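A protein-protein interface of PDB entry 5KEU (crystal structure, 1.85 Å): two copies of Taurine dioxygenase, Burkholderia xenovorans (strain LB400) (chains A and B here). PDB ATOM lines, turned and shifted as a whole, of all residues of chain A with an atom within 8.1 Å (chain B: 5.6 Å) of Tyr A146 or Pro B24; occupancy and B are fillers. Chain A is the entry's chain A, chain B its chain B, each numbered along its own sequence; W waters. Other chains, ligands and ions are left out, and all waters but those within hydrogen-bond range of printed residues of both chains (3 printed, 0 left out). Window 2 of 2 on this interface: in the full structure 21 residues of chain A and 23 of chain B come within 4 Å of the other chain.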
ATOM      1  N   ILE A 143      27.598  12.898 -30.672  1.00  0.00           N
ATOM      2  CA  ILE A 143      26.468  12.113 -30.194  1.00  0.00           C
ATOM      3  C   ILE A 143      26.974  10.875 -29.464  1.00  0.00           C
ATOM      4  O   ILE A 143      27.747  10.097 -30.032  1.00  0.00           O
ATOM      5  CB  ILE A 143      25.508  11.717 -31.330  1.00  0.00           C
ATOM      6  CG1 ILE A 143      24.862  12.974 -31.921  1.00  0.00           C
ATOM      7  CG2 ILE A 143      24.436  10.732 -30.816  1.00  0.00           C
ATOM      8  CD1 ILE A 143      23.978  13.742 -30.928  1.00  0.00           C
ATOM      9  N   PRO A 144      26.586  10.669 -28.205  1.00  0.00           N
ATOM     10  CA  PRO A 144      27.062   9.504 -27.465  1.00  0.00           C
ATOM     11  C   PRO A 144      26.641   8.220 -28.151  1.00  0.00           C
ATOM     12  O   PRO A 144      25.550   8.142 -28.752  1.00  0.00           O
ATOM     13  CB  PRO A 144      26.375   9.647 -26.098  1.00  0.00           C
ATOM     14  CG  PRO A 144      25.954  11.061 -25.991  1.00  0.00           C
ATOM     15  CD  PRO A 144      25.709  11.541 -27.405  1.00  0.00           C
ATOM     16  N   PRO A 145      27.449   7.168 -28.034  1.00  0.00           N
ATOM     17  CA  PRO A 145      27.015   5.829 -28.482  1.00  0.00           C
ATOM     18  C   PRO A 145      25.695   5.392 -27.900  1.00  0.00           C
ATOM     19  O   PRO A 145      24.939   4.662 -28.557  1.00  0.00           O
ATOM     20  CB  PRO A 145      28.149   4.917 -27.986  1.00  0.00           C
ATOM     21  CG  PRO A 145      29.346   5.822 -27.905  1.00  0.00           C
ATOM     22  CD  PRO A 145      28.825   7.170 -27.505  1.00  0.00           C
ATOM     23  N   TYR A 146      25.420   5.781 -26.660  1.00  0.00           N
ATOM     24  CA  TYR A 146      24.131   5.539 -26.034  1.00  0.00           C
ATOM     25  C   TYR A 146      23.938   6.583 -24.950  1.00  0.00           C
ATOM     26  O   TYR A 146      24.903   7.192 -24.471  1.00  0.00           O
ATOM     27  CB  TYR A 146      24.025   4.120 -25.461  1.00  0.00           C
ATOM     28  CG  TYR A 146      25.183   3.703 -24.578  1.00  0.00           C
ATOM     29  CD1 TYR A 146      25.096   3.811 -23.190  1.00  0.00           C
ATOM     30  CD2 TYR A 146      26.346   3.176 -25.127  1.00  0.00           C
ATOM     31  CE1 TYR A 146      26.152   3.411 -22.372  1.00  0.00           C
ATOM     32  CE2 TYR A 146      27.401   2.778 -24.320  1.00  0.00           C
ATOM     33  CZ  TYR A 146      27.294   2.902 -22.946  1.00  0.00           C
ATOM     34  OH  TYR A 146      28.338   2.512 -22.145  1.00  0.00           O
ATOM     35  N   GLY A 147      22.679   6.768 -24.561  1.00  0.00           N
ATOM     36  CA  GLY A 147      22.284   7.848 -23.673  1.00  0.00           C
ATOM     37  C   GLY A 147      21.918   9.091 -24.454  1.00  0.00           C
ATOM     38  O   GLY A 147      22.416   9.339 -25.548  1.00  0.00           O
ATOM     39  N   GLY A 148      21.003   9.876 -23.894  1.00  0.00           N
ATOM     40  CA  GLY A 148      20.673  11.162 -24.490  1.00  0.00           C
ATOM     41  C   GLY A 148      19.523  11.164 -25.473  1.00  0.00           C
ATOM     42  O   GLY A 148      19.432  12.090 -26.292  1.00  0.00           O
ATOM     43  N   ASP A 149      18.640  10.164 -25.426  1.00  0.00           N
ATOM     44  CA  ASP A 149      17.482  10.173 -26.313  1.00  0.00           C
ATOM     45  C   ASP A 149      16.572  11.364 -26.005  1.00  0.00           C
ATOM     46  O   ASP A 149      16.495  11.843 -24.870  1.00  0.00           O
ATOM     47  CB  ASP A 149      16.669   8.879 -26.158  1.00  0.00           C
ATOM     48  CG  ASP A 149      17.409   7.624 -26.635  1.00  0.00           C
ATOM     49  OD1 ASP A 149      18.583   7.712 -27.047  1.00  0.00           O
ATOM     50  OD2 ASP A 149      16.794   6.527 -26.561  1.00  0.00           O
ATOM     51  N   LYS A 257      16.559   7.952 -30.670  1.00  0.00           N
ATOM     52  CA  LYS A 257      17.971   7.786 -30.344  1.00  0.00           C
ATOM     53  C   LYS A 257      18.809   8.500 -31.399  1.00  0.00           C
ATOM     54  O   LYS A 257      18.780   8.135 -32.585  1.00  0.00           O
ATOM     55  CB  LYS A 257      18.349   6.306 -30.265  1.00  0.00           C
ATOM     56  CG  LYS A 257      19.795   6.089 -29.811  1.00  0.00           C
ATOM     57  CD  LYS A 257      20.074   4.600 -29.644  1.00  0.00           C
ATOM     58  CE  LYS A 257      21.484   4.353 -29.073  1.00  0.00           C
ATOM     59  NZ  LYS A 257      22.548   4.996 -29.904  1.00  0.00           N
ATOM     60  N   TRP A 258      19.553   9.517 -30.963  1.00  0.00           N
ATOM     61  CA  TRP A 258      20.386  10.301 -31.858  1.00  0.00           C
ATOM     62  C   TRP A 258      21.547   9.481 -32.399  1.00  0.00           C
ATOM     63  O   TRP A 258      22.043   8.547 -31.759  1.00  0.00           O
ATOM     64  CB  TRP A 258      20.936  11.536 -31.131  1.00  0.00           C
ATOM     65  CG  TRP A 258      19.835  12.496 -30.771  1.00  0.00           C
ATOM     66  CD1 TRP A 258      19.087  12.505 -29.616  1.00  0.00           C
ATOM     67  CD2 TRP A 258      19.350  13.574 -31.576  1.00  0.00           C
ATOM     68  NE1 TRP A 258      18.170  13.535 -29.665  1.00  0.00           N
ATOM     69  CE2 TRP A 258      18.312  14.202 -30.856  1.00  0.00           C
ATOM     70  CE3 TRP A 258      19.702  14.077 -32.835  1.00  0.00           C
ATOM     71  CZ2 TRP A 258      17.610  15.295 -31.360  1.00  0.00           C
ATOM     72  CZ3 TRP A 258      19.006  15.160 -33.333  1.00  0.00           C
ATOM     73  CH2 TRP A 258      17.963  15.757 -32.597  1.00  0.00           C
ATOM     74  N   ASP A 278      19.303  10.998 -18.674  1.00  0.00           N
ATOM     75  CA  ASP A 278      20.153   9.823 -18.455  1.00  0.00           C
ATOM     76  C   ASP A 278      21.593  10.081 -18.875  1.00  0.00           C
ATOM     77  O   ASP A 278      22.501   9.381 -18.408  1.00  0.00           O
ATOM     78  CB  ASP A 278      19.574   8.568 -19.155  1.00  0.00           C
ATOM     79  CG  ASP A 278      19.787   8.540 -20.691  1.00  0.00           C
ATOM     80  OD1 ASP A 278      19.930   9.609 -21.318  1.00  0.00           O
ATOM     81  OD2 ASP A 278      19.776   7.417 -21.277  1.00  0.00           O
ATOM     82  N   ILE A 279      21.833  11.114 -19.687  1.00  0.00           N
ATOM     83  CA  ILE A 279      23.165  11.366 -20.230  1.00  0.00           C
ATOM     84  C   ILE A 279      24.119  11.940 -19.191  1.00  0.00           C
ATOM     85  O   ILE A 279      25.342  11.931 -19.396  1.00  0.00           O
ATOM     86  CB  ILE A 279      23.048  12.286 -21.463  1.00  0.00           C
ATOM     87  CG1 ILE A 279      24.355  12.310 -22.261  1.00  0.00           C
ATOM     88  CG2 ILE A 279      22.609  13.694 -21.053  1.00  0.00           C
ATOM     89  CD1 ILE A 279      24.879  10.929 -22.623  1.00  0.00           C
ATOM     90  N   ASP A 281      24.796  10.679 -16.373  1.00  0.00           N
ATOM     91  CA  ASP A 281      25.431   9.531 -15.742  1.00  0.00           C
ATOM     92  C   ASP A 281      26.586   8.955 -16.548  1.00  0.00           C
ATOM     93  O   ASP A 281      27.197   7.979 -16.102  1.00  0.00           O
ATOM     94  CB  ASP A 281      24.380   8.442 -15.497  1.00  0.00           C
ATOM     95  CG  ASP A 281      23.320   8.876 -14.508  1.00  0.00           C
ATOM     96  OD1 ASP A 281      23.245  10.088 -14.219  1.00  0.00           O
ATOM     97  OD2 ASP A 281      22.567   8.017 -14.008  1.00  0.00           O
ATOM     98  N   LEU A 282      26.910   9.513 -17.712  1.00  0.00           N
ATOM     99  CA  LEU A 282      27.901   8.915 -18.594  1.00  0.00           C
ATOM    100  C   LEU A 282      28.976   9.934 -18.957  1.00  0.00           C
ATOM    101  O   LEU A 282      28.726  11.143 -18.975  1.00  0.00           O
ATOM    102  CB  LEU A 282      27.241   8.382 -19.875  1.00  0.00           C
ATOM    103  CG  LEU A 282      26.043   7.437 -19.689  1.00  0.00           C
ATOM    104  CD1 LEU A 282      25.322   7.236 -21.019  1.00  0.00           C
ATOM    105  CD2 LEU A 282      26.499   6.104 -19.113  1.00  0.00           C
ATOM    106  N   ASP A 283      30.165   9.442 -19.304  1.00  0.00           N
ATOM    107  CA  ASP A 283      31.280  10.332 -19.628  1.00  0.00           C
ATOM    108  C   ASP A 283      31.218  10.913 -21.040  1.00  0.00           C
ATOM    109  O   ASP A 283      32.025  11.794 -21.364  1.00  0.00           O
ATOM    110  CB  ASP A 283      32.606   9.591 -19.441  1.00  0.00           C
ATOM    111  CG  ASP A 283      32.830   9.152 -18.005  1.00  0.00           C
ATOM    112  OD1 ASP A 283      32.293   9.817 -17.090  1.00  0.00           O
ATOM    113  OD2 ASP A 283      33.544   8.147 -17.795  1.00  0.00           O
ATOM    114  N   PHE A 284      30.274  10.464 -21.864  1.00  0.00           N
ATOM    115  CA  PHE A 284      30.243  10.785 -23.281  1.00  0.00           C
ATOM    116  C   PHE A 284      29.907  12.256 -23.478  1.00  0.00           C
ATOM    117  O   PHE A 284      28.975  12.773 -22.862  1.00  0.00           O
ATOM    118  CB  PHE A 284      29.169   9.970 -24.005  1.00  0.00           C
ATOM    119  CG  PHE A 284      29.374   8.488 -23.976  1.00  0.00           C
ATOM    120  CD1 PHE A 284      30.593   7.931 -24.300  1.00  0.00           C
ATOM    121  CD2 PHE A 284      28.312   7.648 -23.666  1.00  0.00           C
ATOM    122  CE1 PHE A 284      30.766   6.560 -24.300  1.00  0.00           C
ATOM    123  CE2 PHE A 284      28.474   6.273 -23.669  1.00  0.00           C
ATOM    124  CZ  PHE A 284      29.703   5.732 -23.974  1.00  0.00           C
ATOM    125  N   ASP A 285      30.627  12.915 -24.380  1.00  0.00           N
ATOM    126  CA  ASP A 285      30.268  14.281 -24.747  1.00  0.00           C
ATOM    127  C   ASP A 285      28.987  14.274 -25.577  1.00  0.00           C
ATOM    128  O   ASP A 285      28.648  13.281 -26.226  1.00  0.00           O
ATOM    129  CB  ASP A 285      31.426  14.923 -25.524  1.00  0.00           C
ATOM    130  CG  ASP A 285      31.292  16.444 -25.666  1.00  0.00           C
ATOM    131  OD1 ASP A 285      32.186  17.025 -26.313  1.00  0.00           O
ATOM    132  OD2 ASP A 285      30.318  17.047 -25.151  1.00  0.00           O
ATOM    133  N   ARG A 286      28.250  15.388 -25.545  1.00  0.00           N
ATOM    134  CA  ARG A 286      27.024  15.470 -26.331  1.00  0.00           C
ATOM    135  C   ARG A 286      26.865  16.903 -26.807  1.00  0.00           C
ATOM    136  O   ARG A 286      26.818  17.821 -25.985  1.00  0.00           O
ATOM    137  CB  ARG A 286      25.801  15.019 -25.512  1.00  0.00           C
ATOM    138  CG  ARG A 286      24.490  14.938 -26.298  1.00  0.00           C
ATOM    139  CD  ARG A 286      23.399  14.292 -25.440  1.00  0.00           C
ATOM    140  NE  ARG A 286      22.111  14.186 -26.114  1.00  0.00           N
ATOM    141  CZ  ARG A 286      21.194  15.144 -26.119  1.00  0.00           C
ATOM    142  NH1 ARG A 286      21.452  16.286 -25.492  1.00  0.00           N
ATOM    143  NH2 ARG A 286      20.029  14.964 -26.746  1.00  0.00           N
ATOM    144  N   VAL B  22      27.998  -6.091 -28.316  1.00  0.00           N
ATOM    145  CA  VAL B  22      26.980  -5.602 -27.383  1.00  0.00           C
ATOM    146  C   VAL B  22      26.842  -4.093 -27.576  1.00  0.00           C
ATOM    147  O   VAL B  22      27.782  -3.340 -27.297  1.00  0.00           O
ATOM    148  CB  VAL B  22      27.327  -5.932 -25.922  1.00  0.00           C
ATOM    149  CG1 VAL B  22      26.267  -5.326 -24.957  1.00  0.00           C
ATOM    150  CG2 VAL B  22      27.427  -7.435 -25.718  1.00  0.00           C
ATOM    151  N   LYS B  23      25.678  -3.644 -28.058  1.00  0.00           N
ATOM    152  CA  LYS B  23      25.423  -2.220 -28.302  1.00  0.00           C
ATOM    153  C   LYS B  23      24.370  -1.697 -27.332  1.00  0.00           C
ATOM    154  O   LYS B  23      23.164  -1.852 -27.586  1.00  0.00           O
ATOM    155  CB  LYS B  23      24.966  -1.982 -29.743  1.00  0.00           C
ATOM    156  CG  LYS B  23      25.987  -2.293 -30.808  1.00  0.00           C
ATOM    157  CD  LYS B  23      25.411  -1.987 -32.186  1.00  0.00           C
ATOM    158  CE  LYS B  23      24.756  -0.618 -32.229  1.00  0.00           C
ATOM    159  NZ  LYS B  23      24.007  -0.400 -33.500  1.00  0.00           N
ATOM    160  N   PRO B  24      24.763  -1.064 -26.224  1.00  0.00           N
ATOM    161  CA  PRO B  24      23.769  -0.549 -25.271  1.00  0.00           C
ATOM    162  C   PRO B  24      22.846   0.486 -25.909  1.00  0.00           C
ATOM    163  O   PRO B  24      23.228   1.211 -26.830  1.00  0.00           O
ATOM    164  CB  PRO B  24      24.625   0.078 -24.167  1.00  0.00           C
ATOM    165  CG  PRO B  24      25.987  -0.616 -24.302  1.00  0.00           C
ATOM    166  CD  PRO B  24      26.153  -0.868 -25.767  1.00  0.00           C
ATOM    167  N   LEU B  25      21.622   0.558 -25.394  1.00  0.00           N
ATOM    168  CA  LEU B  25      20.595   1.410 -25.981  1.00  0.00           C
ATOM    169  C   LEU B  25      20.197   2.600 -25.122  1.00  0.00           C
ATOM    170  O   LEU B  25      19.479   3.483 -25.615  1.00  0.00           O
ATOM    171  CB  LEU B  25      19.349   0.575 -26.306  1.00  0.00           C
ATOM    172  CG  LEU B  25      19.621  -0.415 -27.435  1.00  0.00           C
ATOM    173  CD1 LEU B  25      18.465  -1.427 -27.572  1.00  0.00           C
ATOM    174  CD2 LEU B  25      19.896   0.290 -28.745  1.00  0.00           C
ATOM    175  N   SER B  26      20.649   2.663 -23.874  1.00  0.00           N
ATOM    176  CA  SER B  26      20.407   3.801 -22.991  1.00  0.00           C
ATOM    177  C   SER B  26      21.478   3.746 -21.914  1.00  0.00           C
ATOM    178  O   SER B  26      22.310   2.842 -21.905  1.00  0.00           O
ATOM    179  CB  SER B  26      18.998   3.775 -22.390  1.00  0.00           C
ATOM    180  OG  SER B  26      18.899   2.797 -21.361  1.00  0.00           O
ATOM    181  N   ALA B  27      21.455   4.711 -20.994  1.00  0.00           N
ATOM    182  CA  ALA B  27      22.522   4.759 -19.999  1.00  0.00           C
ATOM    183  C   ALA B  27      22.539   3.501 -19.136  1.00  0.00           C
ATOM    184  O   ALA B  27      23.616   3.014 -18.762  1.00  0.00           O
ATOM    185  CB  ALA B  27      22.381   6.000 -19.117  1.00  0.00           C
ATOM    186  N   GLY B  30      19.081  -1.968 -21.634  1.00  0.00           N
ATOM    187  CA  GLY B  30      18.847  -2.345 -23.009  1.00  0.00           C
ATOM    188  C   GLY B  30      20.126  -2.450 -23.809  1.00  0.00           C
ATOM    189  O   GLY B  30      20.967  -1.543 -23.758  1.00  0.00           O
ATOM    190  N   ALA B  31      20.282  -3.533 -24.570  1.00  0.00           N
ATOM    191  CA  ALA B  31      21.420  -3.644 -25.471  1.00  0.00           C
ATOM    192  C   ALA B  31      21.058  -4.546 -26.642  1.00  0.00           C
ATOM    193  O   ALA B  31      20.409  -5.584 -26.478  1.00  0.00           O
ATOM    194  CB  ALA B  31      22.674  -4.178 -24.748  1.00  0.00           C
ATOM    195  N   GLU B  32      21.480  -4.131 -27.828  1.00  0.00           N
ATOM    196  CA  GLU B  32      21.294  -4.920 -29.031  1.00  0.00           C
ATOM    197  C   GLU B  32      22.538  -5.774 -29.238  1.00  0.00           C
ATOM    198  O   GLU B  32      23.664  -5.266 -29.148  1.00  0.00           O
ATOM    199  CB  GLU B  32      21.049  -3.994 -30.223  1.00  0.00           C
ATOM    200  CG  GLU B  32      20.461  -4.669 -31.428  1.00  0.00           C
ATOM    201  CD  GLU B  32      20.004  -3.658 -32.466  1.00  0.00           C
ATOM    202  OE1 GLU B  32      20.849  -3.240 -33.285  1.00  0.00           O
ATOM    203  OE2 GLU B  32      18.808  -3.273 -32.439  1.00  0.00           O
ATOM    204  N   TRP B  57      22.616  -5.501 -18.753  1.00  0.00           N
ATOM    205  CA  TRP B  57      21.754  -4.554 -19.445  1.00  0.00           C
ATOM    206  C   TRP B  57      20.266  -4.850 -19.277  1.00  0.00           C
ATOM    207  O   TRP B  57      19.438  -4.074 -19.781  1.00  0.00           O
ATOM    208  CB  TRP B  57      22.147  -4.490 -20.933  1.00  0.00           C
ATOM    209  CG  TRP B  57      23.502  -3.805 -21.101  1.00  0.00           C
ATOM    210  CD1 TRP B  57      24.685  -4.387 -21.443  1.00  0.00           C
ATOM    211  CD2 TRP B  57      23.789  -2.419 -20.867  1.00  0.00           C
ATOM    212  NE1 TRP B  57      25.697  -3.439 -21.454  1.00  0.00           N
ATOM    213  CE2 TRP B  57      25.166  -2.226 -21.107  1.00  0.00           C
ATOM    214  CE3 TRP B  57      23.009  -1.316 -20.501  1.00  0.00           C
ATOM    215  CZ2 TRP B  57      25.784  -0.976 -20.975  1.00  0.00           C
ATOM    216  CZ3 TRP B  57      23.622  -0.070 -20.378  1.00  0.00           C
ATOM    217  CH2 TRP B  57      25.001   0.083 -20.610  1.00  0.00           C
HETATM  218  O   HOH W   1      17.318   4.033 -27.076  1.00  0.00           O
HETATM  219  O   HOH W   2      20.262   6.042 -25.917  1.00  0.00           O
HETATM  220  O   HOH W   3      25.295   1.677 -28.520  1.00  0.00           O
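O of Pro B24 touches CB of Tyr A146, at 3.3 Å. Tyr A146 touches Ser B26 (CD1 to O, 3.2 Å). Trp B57 touches Tyr A146 (CH2 to CE1, 3.9 Å). Ser B26 touches Asp A278 (CB to OD2, 3.9 Å). Ala B27 touches Leu A282.
The side-chain carboxylate (OD2) of Asp A278 sits at hydrogen-bond distance from the backbone NH (N) of Ala B27, at 3.2 Å.
No position is printed for both chains.
Water W1 lies within hydrogen-bond range of the side-chain carboxylate of Asp A149 and the backbone carbonyl oxygen of Leu B25. Water W2 lies within hydrogen-bond range of OD1 of Asp A149 (2.6 Å), O of Leu B25 (2.7 Å) and N of Gly A147 (2.9 Å). Water W3 bridges the backbone carbonyl oxygen of Pro B24 (2.7 Å) and the backbone carbonyl oxygen of Pro A145 (3.0 Å).
Of chain B, only Pro B24 (3.3 Å), Ser B26 (3.2 Å) and Trp B57 (3.9 Å) come within 4 Å of Tyr A146. Printed residues of chain B within 4 Å of Asp A278: Ser B26 (3.9 Å) and Ala B27 (3.2 Å). Printed residues of chain B within 4 Å of Leu A282: Ala B27. Printed residues of chain A within 4 Å of Pro B24: Tyr A146 (3.3 Å). Gly B30 touches none of the printed residues of chain A. The nearest printed residue of chain A that does not touch Pro B24 is Pro A145 (4.2 Å). The nearest printed residue of chain B that does not touch Leu A282 is Ser B26 (5.3 Å).
Of the 17 printed residues of chain A, 3 touch a printed residue of chain B. Of the 10 printed residues of chain B, 4 touch a printed residue of chain A. Among the printed residues, no Asp or Glu carboxylate lies within 4 Å of a Lys or Arg side-chain nitrogen of the other chain.
The backbone NH (N) of Gly A148 lies within hydrogen-bond range of the side-chain carboxylate (OD1) of Asp A278, at 2.8 Å. The backbone NH (N) of Gly B30 sits at hydrogen-bond distance from the backbone carbonyl oxygen (O) of Trp B57 (2.8 Å).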
